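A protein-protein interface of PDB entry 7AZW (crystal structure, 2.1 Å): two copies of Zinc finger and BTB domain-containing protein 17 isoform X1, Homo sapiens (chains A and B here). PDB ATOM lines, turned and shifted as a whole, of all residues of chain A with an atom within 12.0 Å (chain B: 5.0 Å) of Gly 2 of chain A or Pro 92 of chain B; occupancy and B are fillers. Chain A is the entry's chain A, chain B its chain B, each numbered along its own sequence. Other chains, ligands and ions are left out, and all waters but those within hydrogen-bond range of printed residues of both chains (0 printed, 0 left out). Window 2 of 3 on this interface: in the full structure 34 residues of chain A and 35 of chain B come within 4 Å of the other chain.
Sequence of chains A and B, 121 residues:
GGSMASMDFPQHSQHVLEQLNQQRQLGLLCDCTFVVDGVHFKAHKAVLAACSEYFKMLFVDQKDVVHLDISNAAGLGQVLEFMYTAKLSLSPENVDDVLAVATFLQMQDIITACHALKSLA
No position is printed for both chains.
Of the 6 pairs that touch across the chains among the printed residues, none has its exchanged pair printed and touching as well.
CA of Gly 2 of chain A touches CG of Pro 92 of chain B, at 3.6 Å.
Pro 92 of chain B touches Ser 3 of chain A.
Ser 3 of chain A touches Leu 117 of chain B.
Met 4 of chain A touches Leu 90 of chain B.
Ser 91 of chain B touches Met 4 of chain A (CB to CG, 3.7 Å).
OG of Ser 91 of chain B lies close to N of Glu 93 of chain B (3.4 Å).
The backbone NH (N) of Ser 91 of chain B sits at hydrogen-bond distance from the side-chain amide oxygen (OD1) of Asn 94 of chain B, at 2.8 Å.
The backbone NH of Leu 90 of chain B sits at hydrogen-bond distance from the backbone carbonyl oxygen of Ala 5 of chain A (2.8 Å).
Of the 6 printed residues of chain A, 4 touch a printed residue of chain B.
Gly 2 of chain A touches one residue of chain B.
Printed residues of chain B within 4 Å of Ser 3 of chain A: Pro 92 and Leu 117.
Of the printed residues of chain B, Ala 5 of chain A touches Leu 90 (2.8 Å).
Met 7 of chain A touches none of the printed residues of chain B.
Of the printed residues of chain A, Leu 90 of chain B touches Met 4 and Ala 5.
Of chain A, only Gly 2 and Ser 3 come within 4 Å of Pro 92 of chain B.
No residue of chain A comes within 4 Å of Glu 93 of chain B.
No residue of chain A comes within 4 Å of Asn 94 of chain B.
No residue of chain A comes within 4 Å of Val 95 of chain B.
The nearest printed residue of chain B that does not touch Gly 2 of chain A is Ser 91 of chain B (6.6 Å).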
ATOM      1  N   GLY A   2     -23.129 -12.264   7.819  1.00  0.00           N
ATOM      2  CA  GLY A   2     -22.671 -10.888   7.873  1.00  0.00           C
ATOM      3  C   GLY A   2     -23.176 -10.147   9.094  1.00  0.00           C
ATOM      4  O   GLY A   2     -23.766  -9.073   8.981  1.00  0.00           O
ATOM      5  N   SER A   3     -22.936 -10.723  10.268  1.00  0.00           N
ATOM      6  CA  SER A   3     -23.455 -10.173  11.510  1.00  0.00           C
ATOM      7  C   SER A   3     -22.554  -9.061  12.034  1.00  0.00           C
ATOM      8  O   SER A   3     -21.332  -9.091  11.872  1.00  0.00           O
ATOM      9  CB  SER A   3     -23.587 -11.269  12.568  1.00  0.00           C
ATOM     10  OG  SER A   3     -24.765 -12.030  12.374  1.00  0.00           O
ATOM     11  N   MET A   4     -23.175  -8.077  12.678  1.00  0.00           N
ATOM     12  CA  MET A   4     -22.472  -6.967  13.304  1.00  0.00           C
ATOM     13  C   MET A   4     -22.704  -7.011  14.807  1.00  0.00           C
ATOM     14  O   MET A   4     -23.815  -7.303  15.263  1.00  0.00           O
ATOM     15  CB  MET A   4     -22.939  -5.626  12.731  1.00  0.00           C
ATOM     16  CG  MET A   4     -22.806  -5.530  11.220  1.00  0.00           C
ATOM     17  SD  MET A   4     -23.390  -3.961  10.551  1.00  0.00           S
ATOM     18  CE  MET A   4     -25.113  -4.007  11.035  1.00  0.00           C
ATOM     19  N   ALA A   5     -21.656  -6.722  15.576  1.00  0.00           N
ATOM     20  CA  ALA A   5     -21.702  -6.825  17.029  1.00  0.00           C
ATOM     21  C   ALA A   5     -21.180  -5.538  17.647  1.00  0.00           C
ATOM     22  O   ALA A   5     -20.026  -5.159  17.415  1.00  0.00           O
ATOM     23  CB  ALA A   5     -20.888  -8.024  17.524  1.00  0.00           C
ATOM     24  N   SER A   6     -22.026  -4.872  18.428  1.00  0.00           N
ATOM     25  CA  SER A   6     -21.617  -3.720  19.225  1.00  0.00           C
ATOM     26  C   SER A   6     -21.252  -4.223  20.617  1.00  0.00           C
ATOM     27  O   SER A   6     -22.134  -4.557  21.416  1.00  0.00           O
ATOM     28  CB  SER A   6     -22.728  -2.675  19.284  1.00  0.00           C
ATOM     29  OG  SER A   6     -22.982  -2.128  18.003  1.00  0.00           O
ATOM     30  N   MET A   7     -19.957  -4.284  20.906  1.00  0.00           N
ATOM     31  CA  MET A   7     -19.460  -4.877  22.138  1.00  0.00           C
ATOM     32  C   MET A   7     -19.234  -3.813  23.206  1.00  0.00           C
ATOM     33  O   MET A   7     -18.844  -2.681  22.913  1.00  0.00           O
ATOM     34  CB  MET A   7     -18.158  -5.638  21.884  1.00  0.00           C
ATOM     35  CG  MET A   7     -18.227  -6.604  20.713  1.00  0.00           C
ATOM     36  SD  MET A   7     -16.868  -7.786  20.720  1.00  0.00           S
ATOM     37  CE  MET A   7     -17.186  -8.659  22.252  1.00  0.00           C
ATOM     38  N   LEU B  90     -17.845  -4.226  15.957  1.00  0.00           N
ATOM     39  CA  LEU B  90     -17.227  -5.060  14.937  1.00  0.00           C
ATOM     40  C   LEU B  90     -18.239  -5.398  13.851  1.00  0.00           C
ATOM     41  O   LEU B  90     -19.427  -5.578  14.128  1.00  0.00           O
ATOM     42  CB  LEU B  90     -16.675  -6.341  15.560  1.00  0.00           C
ATOM     43  CG  LEU B  90     -15.513  -6.174  16.543  1.00  0.00           C
ATOM     44  CD1 LEU B  90     -15.107  -7.521  17.119  1.00  0.00           C
ATOM     45  CD2 LEU B  90     -14.327  -5.500  15.866  1.00  0.00           C
ATOM     46  N   SER B  91     -17.759  -5.489  12.616  1.00  0.00           N
ATOM     47  CA  SER B  91     -18.590  -5.828  11.470  1.00  0.00           C
ATOM     48  C   SER B  91     -17.725  -6.556  10.464  1.00  0.00           C
ATOM     49  O   SER B  91     -16.492  -6.445  10.500  1.00  0.00           O
ATOM     50  CB  SER B  91     -19.218  -4.577  10.841  1.00  0.00           C
ATOM     51  OG  SER B  91     -18.247  -3.805  10.158  1.00  0.00           O
ATOM     52  N   PRO B  92     -18.328  -7.331   9.552  1.00  0.00           N
ATOM     53  CA  PRO B  92     -17.524  -8.003   8.519  1.00  0.00           C
ATOM     54  C   PRO B  92     -16.719  -7.045   7.659  1.00  0.00           C
ATOM     55  O   PRO B  92     -15.747  -7.475   7.025  1.00  0.00           O
ATOM     56  CB  PRO B  92     -18.575  -8.754   7.690  1.00  0.00           C
ATOM     57  CG  PRO B  92     -19.722  -8.939   8.622  1.00  0.00           C
ATOM     58  CD  PRO B  92     -19.751  -7.715   9.479  1.00  0.00           C
ATOM     59  N   GLU B  93     -17.082  -5.762   7.626  1.00  0.00           N
ATOM     60  CA  GLU B  93     -16.350  -4.796   6.814  1.00  0.00           C
ATOM     61  C   GLU B  93     -15.064  -4.327   7.484  1.00  0.00           C
ATOM     62  O   GLU B  93     -14.124  -3.928   6.787  1.00  0.00           O
ATOM     63  CB  GLU B  93     -17.241  -3.593   6.503  1.00  0.00           C
ATOM     64  CG  GLU B  93     -16.800  -2.791   5.291  1.00  0.00           C
ATOM     65  CD  GLU B  93     -16.805  -1.298   5.550  1.00  0.00           C
ATOM     66  OE1 GLU B  93     -17.162  -0.891   6.676  1.00  0.00           O
ATOM     67  OE2 GLU B  93     -16.448  -0.530   4.630  1.00  0.00           O
ATOM     68  N   ASN B  94     -14.993  -4.367   8.817  1.00  0.00           N
ATOM     69  CA  ASN B  94     -13.851  -3.826   9.539  1.00  0.00           C
ATOM     70  C   ASN B  94     -13.155  -4.815  10.463  1.00  0.00           C
ATOM     71  O   ASN B  94     -12.115  -4.465  11.032  1.00  0.00           O
ATOM     72  CB  ASN B  94     -14.272  -2.596  10.365  1.00  0.00           C
ATOM     73  CG  ASN B  94     -15.363  -2.908  11.387  1.00  0.00           C
ATOM     74  OD1 ASN B  94     -15.540  -4.051  11.810  1.00  0.00           O
ATOM     75  ND2 ASN B  94     -16.096  -1.878  11.793  1.00  0.00           N
ATOM     76  N   VAL B  95     -13.686  -6.030  10.631  1.00  0.00           N
ATOM     77  CA  VAL B  95     -13.165  -6.937  11.651  1.00  0.00           C
ATOM     78  C   VAL B  95     -11.720  -7.324  11.365  1.00  0.00           C
ATOM     79  O   VAL B  95     -10.928  -7.528  12.295  1.00  0.00           O
ATOM     80  CB  VAL B  95     -14.074  -8.178  11.774  1.00  0.00           C
ATOM     81  CG1 VAL B  95     -14.130  -8.944  10.457  1.00  0.00           C
ATOM     82  CG2 VAL B  95     -13.613  -9.077  12.917  1.00  0.00           C
ATOM     83  N   LEU B 117     -15.975 -12.699  16.168  1.00  0.00           N
ATOM     84  CA  LEU B 117     -16.822 -12.158  15.108  1.00  0.00           C
ATOM     85  C   LEU B 117     -16.684 -12.968  13.824  1.00  0.00           C
ATOM     86  O   LEU B 117     -17.676 -13.201  13.122  1.00  0.00           O
ATOM     87  CB  LEU B 117     -16.472 -10.688  14.863  1.00  0.00           C
ATOM     88  CG  LEU B 117     -17.463  -9.787  14.114  1.00  0.00           C
ATOM     89  CD1 LEU B 117     -17.325  -9.913  12.602  1.00  0.00           C
ATOM     90  CD2 LEU B 117     -18.894 -10.071  14.547  1.00  0.00           C
